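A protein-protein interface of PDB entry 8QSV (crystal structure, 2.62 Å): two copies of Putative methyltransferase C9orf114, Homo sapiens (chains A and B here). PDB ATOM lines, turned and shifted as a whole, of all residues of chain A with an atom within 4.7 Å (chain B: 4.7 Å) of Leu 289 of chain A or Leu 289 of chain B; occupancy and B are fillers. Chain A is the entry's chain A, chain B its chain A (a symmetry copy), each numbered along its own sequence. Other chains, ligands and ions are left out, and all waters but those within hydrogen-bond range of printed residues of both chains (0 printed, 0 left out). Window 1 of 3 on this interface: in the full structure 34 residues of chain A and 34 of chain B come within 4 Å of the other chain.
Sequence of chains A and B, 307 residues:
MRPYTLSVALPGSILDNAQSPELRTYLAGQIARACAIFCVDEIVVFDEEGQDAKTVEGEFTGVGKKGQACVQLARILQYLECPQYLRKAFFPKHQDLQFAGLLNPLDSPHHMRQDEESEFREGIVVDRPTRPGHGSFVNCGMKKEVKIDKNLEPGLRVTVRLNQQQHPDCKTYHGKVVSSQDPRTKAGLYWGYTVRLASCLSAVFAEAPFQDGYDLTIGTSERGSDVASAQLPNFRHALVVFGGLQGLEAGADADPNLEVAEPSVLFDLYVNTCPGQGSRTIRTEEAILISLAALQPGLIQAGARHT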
ATOM      1  N   ALA A  34     -13.931  -0.567  -1.198  1.00  0.00           N
ATOM      2  CA  ALA A  34     -13.975  -1.964  -0.799  1.00  0.00           C
ATOM      3  C   ALA A  34     -14.089  -2.796  -2.068  1.00  0.00           C
ATOM      4  O   ALA A  34     -13.362  -3.766  -2.233  1.00  0.00           O
ATOM      5  CB  ALA A  34     -15.112  -2.217   0.168  1.00  0.00           C
ATOM      6  N   ILE A  37     -11.127  -2.713  -4.303  1.00  0.00           N
ATOM      7  CA  ILE A  37      -9.983  -3.460  -3.814  1.00  0.00           C
ATOM      8  C   ILE A  37     -10.070  -4.897  -4.300  1.00  0.00           C
ATOM      9  O   ILE A  37      -9.062  -5.426  -4.766  1.00  0.00           O
ATOM     10  CB  ILE A  37      -9.836  -3.369  -2.289  1.00  0.00           C
ATOM     11  CG1 ILE A  37      -9.379  -1.965  -1.900  1.00  0.00           C
ATOM     12  CG2 ILE A  37      -8.881  -4.448  -1.773  1.00  0.00           C
ATOM     13  CD1 ILE A  37      -9.632  -1.646  -0.461  1.00  0.00           C
ATOM     14  N   PHE A  38     -11.285  -5.464  -4.232  1.00  0.00           N
ATOM     15  CA  PHE A  38     -11.530  -6.863  -4.543  1.00  0.00           C
ATOM     16  C   PHE A  38     -11.855  -7.079  -6.016  1.00  0.00           C
ATOM     17  O   PHE A  38     -12.324  -8.151  -6.375  1.00  0.00           O
ATOM     18  CB  PHE A  38     -12.638  -7.384  -3.630  1.00  0.00           C
ATOM     19  CG  PHE A  38     -12.087  -7.682  -2.266  1.00  0.00           C
ATOM     20  CD1 PHE A  38     -11.399  -8.859  -2.031  1.00  0.00           C
ATOM     21  CD2 PHE A  38     -12.137  -6.725  -1.259  1.00  0.00           C
ATOM     22  CE1 PHE A  38     -10.831  -9.098  -0.787  1.00  0.00           C
ATOM     23  CE2 PHE A  38     -11.544  -6.959  -0.024  1.00  0.00           C
ATOM     24  CZ  PHE A  38     -10.905  -8.150   0.218  1.00  0.00           C
ATOM     25  N   GLU A 285     -20.541  -1.663   5.360  1.00  0.00           N
ATOM     26  CA  GLU A 285     -19.285  -1.323   4.727  1.00  0.00           C
ATOM     27  C   GLU A 285     -18.145  -2.128   5.337  1.00  0.00           C
ATOM     28  O   GLU A 285     -17.141  -2.344   4.682  1.00  0.00           O
ATOM     29  CB  GLU A 285     -18.993   0.172   4.846  1.00  0.00           C
ATOM     30  CG  GLU A 285     -18.460   0.645   6.184  1.00  0.00           C
ATOM     31  CD  GLU A 285     -19.454   1.043   7.257  1.00  0.00           C
ATOM     32  OE1 GLU A 285     -20.671   0.886   7.043  1.00  0.00           O
ATOM     33  OE2 GLU A 285     -18.982   1.536   8.314  1.00  0.00           O
ATOM     34  N   GLU A 286     -18.277  -2.505   6.606  1.00  0.00           N
ATOM     35  CA  GLU A 286     -17.305  -3.351   7.272  1.00  0.00           C
ATOM     36  C   GLU A 286     -17.466  -4.789   6.792  1.00  0.00           C
ATOM     37  O   GLU A 286     -16.487  -5.495   6.520  1.00  0.00           O
ATOM     38  CB  GLU A 286     -17.521  -3.348   8.790  1.00  0.00           C
ATOM     39  CG  GLU A 286     -17.214  -2.034   9.476  1.00  0.00           C
ATOM     40  CD  GLU A 286     -17.698  -1.951  10.919  1.00  0.00           C
ATOM     41  OE1 GLU A 286     -18.557  -2.772  11.246  1.00  0.00           O
ATOM     42  OE2 GLU A 286     -17.238  -1.051  11.716  1.00  0.00           O
ATOM     43  N   ALA A 287     -18.728  -5.216   6.727  1.00  0.00           N
ATOM     44  CA  ALA A 287     -19.050  -6.589   6.384  1.00  0.00           C
ATOM     45  C   ALA A 287     -18.565  -6.937   4.982  1.00  0.00           C
ATOM     46  O   ALA A 287     -18.116  -8.058   4.764  1.00  0.00           O
ATOM     47  CB  ALA A 287     -20.518  -6.793   6.521  1.00  0.00           C
ATOM     48  N   ILE A 288     -18.618  -5.963   4.058  1.00  0.00           N
ATOM     49  CA  ILE A 288     -18.123  -6.153   2.704  1.00  0.00           C
ATOM     50  C   ILE A 288     -16.629  -6.484   2.686  1.00  0.00           C
ATOM     51  O   ILE A 288     -16.179  -7.338   1.935  1.00  0.00           O
ATOM     52  CB  ILE A 288     -18.421  -4.910   1.848  1.00  0.00           C
ATOM     53  CG1 ILE A 288     -19.913  -4.767   1.554  1.00  0.00           C
ATOM     54  CG2 ILE A 288     -17.621  -4.940   0.557  1.00  0.00           C
ATOM     55  CD1 ILE A 288     -20.267  -3.492   0.811  1.00  0.00           C
ATOM     56  N   LEU A 289     -15.813  -5.753   3.431  1.00  0.00           N
ATOM     57  CA  LEU A 289     -14.397  -6.067   3.440  1.00  0.00           C
ATOM     58  C   LEU A 289     -14.184  -7.452   4.047  1.00  0.00           C
ATOM     59  O   LEU A 289     -13.483  -8.297   3.470  1.00  0.00           O
ATOM     60  CB  LEU A 289     -13.672  -4.981   4.230  1.00  0.00           C
ATOM     61  CG  LEU A 289     -13.584  -3.614   3.539  1.00  0.00           C
ATOM     62  CD1 LEU A 289     -12.959  -2.582   4.454  1.00  0.00           C
ATOM     63  CD2 LEU A 289     -12.780  -3.703   2.250  1.00  0.00           C
ATOM     64  N   ILE A 290     -14.840  -7.713   5.188  1.00  0.00           N
ATOM     65  CA  ILE A 290     -14.649  -8.996   5.844  1.00  0.00           C
ATOM     66  C   ILE A 290     -15.107 -10.125   4.928  1.00  0.00           C
ATOM     67  O   ILE A 290     -14.397 -11.093   4.724  1.00  0.00           O
ATOM     68  CB  ILE A 290     -15.344  -9.070   7.210  1.00  0.00           C
ATOM     69  CG1 ILE A 290     -14.779  -8.046   8.190  1.00  0.00           C
ATOM     70  CG2 ILE A 290     -15.209 -10.467   7.781  1.00  0.00           C
ATOM     71  CD1 ILE A 290     -15.692  -7.734   9.374  1.00  0.00           C
ATOM     72  N   SER A 291     -16.297 -10.005   4.360  1.00  0.00           N
ATOM     73  CA  SER A 291     -16.886 -11.097   3.596  1.00  0.00           C
ATOM     74  C   SER A 291     -16.074 -11.385   2.330  1.00  0.00           C
ATOM     75  O   SER A 291     -15.725 -12.546   2.044  1.00  0.00           O
ATOM     76  CB  SER A 291     -18.315 -10.769   3.300  1.00  0.00           C
ATOM     77  OG  SER A 291     -19.021 -10.494   4.516  1.00  0.00           O
ATOM     78  N   LEU A 292     -15.697 -10.314   1.621  1.00  0.00           N
ATOM     79  CA  LEU A 292     -14.991 -10.477   0.363  1.00  0.00           C
ATOM     80  C   LEU A 292     -13.610 -11.080   0.573  1.00  0.00           C
ATOM     81  O   LEU A 292     -13.169 -11.883  -0.246  1.00  0.00           O
ATOM     82  CB  LEU A 292     -14.938  -9.146  -0.384  1.00  0.00           C
ATOM     83  CG  LEU A 292     -16.278  -8.779  -1.014  1.00  0.00           C
ATOM     84  CD1 LEU A 292     -16.156  -7.584  -1.942  1.00  0.00           C
ATOM     85  CD2 LEU A 292     -16.853  -9.965  -1.761  1.00  0.00           C
ATOM     86  N   ALA A 293     -12.957 -10.752   1.684  1.00  0.00           N
ATOM     87  CA  ALA A 293     -11.708 -11.430   1.988  1.00  0.00           C
ATOM     88  C   ALA A 293     -12.000 -12.877   2.361  1.00  0.00           C
ATOM     89  O   ALA A 293     -11.350 -13.804   1.863  1.00  0.00           O
ATOM     90  CB  ALA A 293     -10.974 -10.720   3.095  1.00  0.00           C
ATOM     91  N   ALA B  34     -12.810  -2.475  14.233  1.00  0.00           N
ATOM     92  CA  ALA B  34     -12.196  -3.560  13.486  1.00  0.00           C
ATOM     93  C   ALA B  34     -11.661  -4.563  14.497  1.00  0.00           C
ATOM     94  O   ALA B  34     -11.890  -5.757  14.358  1.00  0.00           O
ATOM     95  CB  ALA B  34     -11.121  -3.039  12.557  1.00  0.00           C
ATOM     96  N   ILE B  37     -14.232  -6.346  16.493  1.00  0.00           N
ATOM     97  CA  ILE B  37     -14.973  -7.354  15.758  1.00  0.00           C
ATOM     98  C   ILE B  37     -14.248  -8.687  15.855  1.00  0.00           C
ATOM     99  O   ILE B  37     -14.903  -9.698  16.105  1.00  0.00           O
ATOM    100  CB  ILE B  37     -15.235  -6.939  14.304  1.00  0.00           C
ATOM    101  CG1 ILE B  37     -16.273  -5.820  14.269  1.00  0.00           C
ATOM    102  CG2 ILE B  37     -15.665  -8.146  13.467  1.00  0.00           C
ATOM    103  CD1 ILE B  37     -16.268  -5.058  12.982  1.00  0.00           C
ATOM    104  N   PHE B  38     -12.914  -8.638  15.715  1.00  0.00           N
ATOM    105  CA  PHE B  38     -12.075  -9.825  15.662  1.00  0.00           C
ATOM    106  C   PHE B  38     -11.601 -10.258  17.044  1.00  0.00           C
ATOM    107  O   PHE B  38     -10.697 -11.077  17.138  1.00  0.00           O
ATOM    108  CB  PHE B  38     -10.908  -9.561  14.713  1.00  0.00           C
ATOM    109  CG  PHE B  38     -11.359  -9.698  13.288  1.00  0.00           C
ATOM    110  CD1 PHE B  38     -11.488 -10.949  12.712  1.00  0.00           C
ATOM    111  CD2 PHE B  38     -11.784  -8.586  12.572  1.00  0.00           C
ATOM    112  CE1 PHE B  38     -11.973 -11.074  11.417  1.00  0.00           C
ATOM    113  CE2 PHE B  38     -12.293  -8.719  11.285  1.00  0.00           C
ATOM    114  CZ  PHE B  38     -12.373  -9.959  10.702  1.00  0.00           C
ATOM    115  N   GLU B 285      -6.777   1.127   8.026  1.00  0.00           N
ATOM    116  CA  GLU B 285      -8.016   0.716   8.650  1.00  0.00           C
ATOM    117  C   GLU B 285      -8.736  -0.308   7.783  1.00  0.00           C
ATOM    118  O   GLU B 285      -9.509  -1.097   8.297  1.00  0.00           O
ATOM    119  CB  GLU B 285      -8.927   1.915   8.909  1.00  0.00           C
ATOM    120  CG  GLU B 285      -9.691   2.446   7.712  1.00  0.00           C
ATOM    121  CD  GLU B 285      -9.030   3.497   6.842  1.00  0.00           C
ATOM    122  OE1 GLU B 285      -7.853   3.827   7.080  1.00  0.00           O
ATOM    123  OE2 GLU B 285      -9.731   3.998   5.924  1.00  0.00           O
ATOM    124  N   GLU B 286      -8.531  -0.246   6.470  1.00  0.00           N
ATOM    125  CA  GLU B 286      -9.085  -1.220   5.548  1.00  0.00           C
ATOM    126  C   GLU B 286      -8.295  -2.519   5.644  1.00  0.00           C
ATOM    127  O   GLU B 286      -8.859  -3.621   5.662  1.00  0.00           O
ATOM    128  CB  GLU B 286      -8.983  -0.727   4.100  1.00  0.00           C
ATOM    129  CG  GLU B 286      -9.864   0.457   3.765  1.00  0.00           C
ATOM    130  CD  GLU B 286      -9.551   1.114   2.426  1.00  0.00           C
ATOM    131  OE1 GLU B 286      -8.444   0.858   1.947  1.00  0.00           O
ATOM    132  OE2 GLU B 286     -10.399   1.904   1.866  1.00  0.00           O
ATOM    133  N   ALA B 287      -6.971  -2.365   5.671  1.00  0.00           N
ATOM    134  CA  ALA B 287      -6.071  -3.504   5.662  1.00  0.00           C
ATOM    135  C   ALA B 287      -6.275  -4.380   6.892  1.00  0.00           C
ATOM    136  O   ALA B 287      -6.186  -5.598   6.781  1.00  0.00           O
ATOM    137  CB  ALA B 287      -4.668  -3.016   5.564  1.00  0.00           C
ATOM    138  N   ILE B 288      -6.588  -3.757   8.039  1.00  0.00           N
ATOM    139  CA  ILE B 288      -6.872  -4.488   9.264  1.00  0.00           C
ATOM    140  C   ILE B 288      -8.076  -5.419   9.105  1.00  0.00           C
ATOM    141  O   ILE B 288      -8.070  -6.547   9.578  1.00  0.00           O
ATOM    142  CB  ILE B 288      -7.084  -3.509  10.432  1.00  0.00           C
ATOM    143  CG1 ILE B 288      -5.784  -2.823  10.843  1.00  0.00           C
ATOM    144  CG2 ILE B 288      -7.715  -4.216  11.620  1.00  0.00           C
ATOM    145  CD1 ILE B 288      -5.966  -1.763  11.913  1.00  0.00           C
ATOM    146  N   LEU B 289      -9.170  -4.941   8.530  1.00  0.00           N
ATOM    147  CA  LEU B 289     -10.312  -5.818   8.353  1.00  0.00           C
ATOM    148  C   LEU B 289      -9.947  -6.948   7.393  1.00  0.00           C
ATOM    149  O   LEU B 289     -10.182  -8.130   7.687  1.00  0.00           O
ATOM    150  CB  LEU B 289     -11.479  -4.983   7.834  1.00  0.00           C
ATOM    151  CG  LEU B 289     -12.102  -4.019   8.852  1.00  0.00           C
ATOM    152  CD1 LEU B 289     -13.163  -3.156   8.203  1.00  0.00           C
ATOM    153  CD2 LEU B 289     -12.711  -4.778  10.022  1.00  0.00           C
ATOM    154  N   ILE B 290      -9.312  -6.594   6.266  1.00  0.00           N
ATOM    155  CA  ILE B 290      -8.975  -7.613   5.287  1.00  0.00           C
ATOM    156  C   ILE B 290      -8.022  -8.633   5.901  1.00  0.00           C
ATOM    157  O   ILE B 290      -8.235  -9.828   5.801  1.00  0.00           O
ATOM    158  CB  ILE B 290      -8.398  -7.022   3.994  1.00  0.00           C
ATOM    159  CG1 ILE B 290      -9.405  -6.122   3.283  1.00  0.00           C
ATOM    160  CG2 ILE B 290      -7.955  -8.138   3.069  1.00  0.00           C
ATOM    161  CD1 ILE B 290      -8.787  -5.151   2.279  1.00  0.00           C
ATOM    162  N   SER B 291      -6.967  -8.168   6.551  1.00  0.00           N
ATOM    163  CA  SER B 291      -5.921  -9.059   7.036  1.00  0.00           C
ATOM    164  C   SER B 291      -6.454  -9.988   8.132  1.00  0.00           C
ATOM    165  O   SER B 291      -6.254 -11.216   8.082  1.00  0.00           O
ATOM    166  CB  SER B 291      -4.757  -8.241   7.493  1.00  0.00           C
ATOM    167  OG  SER B 291      -4.311  -7.382   6.437  1.00  0.00           O
ATOM    168  N   LEU B 292      -7.210  -9.409   9.072  1.00  0.00           N
ATOM    169  CA  LEU B 292      -7.701 -10.182  10.199  1.00  0.00           C
ATOM    170  C   LEU B 292      -8.700 -11.241   9.756  1.00  0.00           C
ATOM    171  O   LEU B 292      -8.704 -12.338  10.308  1.00  0.00           O
ATOM    172  CB  LEU B 292      -8.275  -9.249  11.263  1.00  0.00           C
ATOM    173  CG  LEU B 292      -7.185  -8.523  12.047  1.00  0.00           C
ATOM    174  CD1 LEU B 292      -7.752  -7.785  13.247  1.00  0.00           C
ATOM    175  CD2 LEU B 292      -6.114  -9.497  12.491  1.00  0.00           C
ATOM    176  N   ALA B 293      -9.497 -10.946   8.733  1.00  0.00           N
ATOM    177  CA  ALA B 293     -10.349 -11.988   8.187  1.00  0.00           C
ATOM    178  C   ALA B 293      -9.488 -13.017   7.466  1.00  0.00           C
ATOM    179  O   ALA B 293      -9.648 -14.227   7.664  1.00  0.00           O
ATOM    180  CB  ALA B 293     -11.382 -11.399   7.262  1.00  0.00           C
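Glu 286 of chain B touches Ile 37 of chain A. Phe 38 of chain A touches Ile 290 of chain B (CZ to CG1, 3.97 Å). Glu 286 of chain A touches Ile 37 of chain B. CD1 of Leu 289 of chain A touches CD1 of Leu 289 of chain B (3.8 Å). CG1 of Ile 290 of chain A touches CZ of Phe 38 of chain B, 3.97 Å away. O of Ile 290 of chain A touches CB of Ala 293 of chain B (3.95 Å). O of Ile 290 of chain B touches CB of Ala 293 of chain A, 3.95 Å away.
Ile 37 of chain A touches Glu 286 of chain B, and with the chains exchanged Glu 286 of chain A touches Ile 37 of chain B. Phe 38 of chain A touches Ile 290 of chain B, and with the chains exchanged Ile 290 of chain A touches Phe 38 of chain B. Leu 289 of chain A touches its own counterpart, Leu 289 of chain B. Ile 290 of chain A touches Ala 293 of chain B, and with the chains exchanged Ala 293 of chain A touches Ile 290 of chain B. Positions printed for both chains: 34, 37, 38, 285, 286, 287, 288, 289, 290, 291, 292 and 293. Of the 7 pairs that touch across the chains among the printed residues, 7 have their exchanged pair printed and touching as well.
Printed residues of chain B that touch a printed residue of chain A: Ile 37, Phe 38, Glu 286, Leu 289, Ile 290 and Ala 293. Along chain B the printed residues that touch a printed residue of chain A span positions 37 to 293. Hydrophobic or aromatic side chains of chain A within 4 Å of the printed part of chain B: Ile 37, Phe 38, Leu 289, Ile 290 and Ala 293. Among the printed residues, 7 pairs touch across the chains. Among the printed residues, no Asp or Glu carboxylate lies within 4 Å of a Lys or Arg side-chain nitrogen of the other chain.
Of the printed residues of chain B, Ile 37 of chain A touches Glu 286. Leu 289 of chain A touches just one residue of chain B: Leu 289 (3.8 Å). Printed residues of chain A within 4 Å of Ile 37 of chain B: Glu 286. Of the printed residues of chain A, Phe 38 of chain B touches Ile 290. Leu 289 of chain B touches just one residue of chain A: Leu 289. Of the printed residues of chain A, Ile 290 of chain B touches Phe 38 (3.97 Å) and Ala 293 (3.95 Å). Printed residues of chain A within 4 Å of Ala 293 of chain B: Ile 290 (3.95 Å). The nearest printed residue of chain B that does not touch Leu 289 of chain A is Ile 290 of chain B (4.2 Å). The nearest printed residue of chain B that does not touch Ile 37 of chain A is Ile 290 of chain B (4.1 Å).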
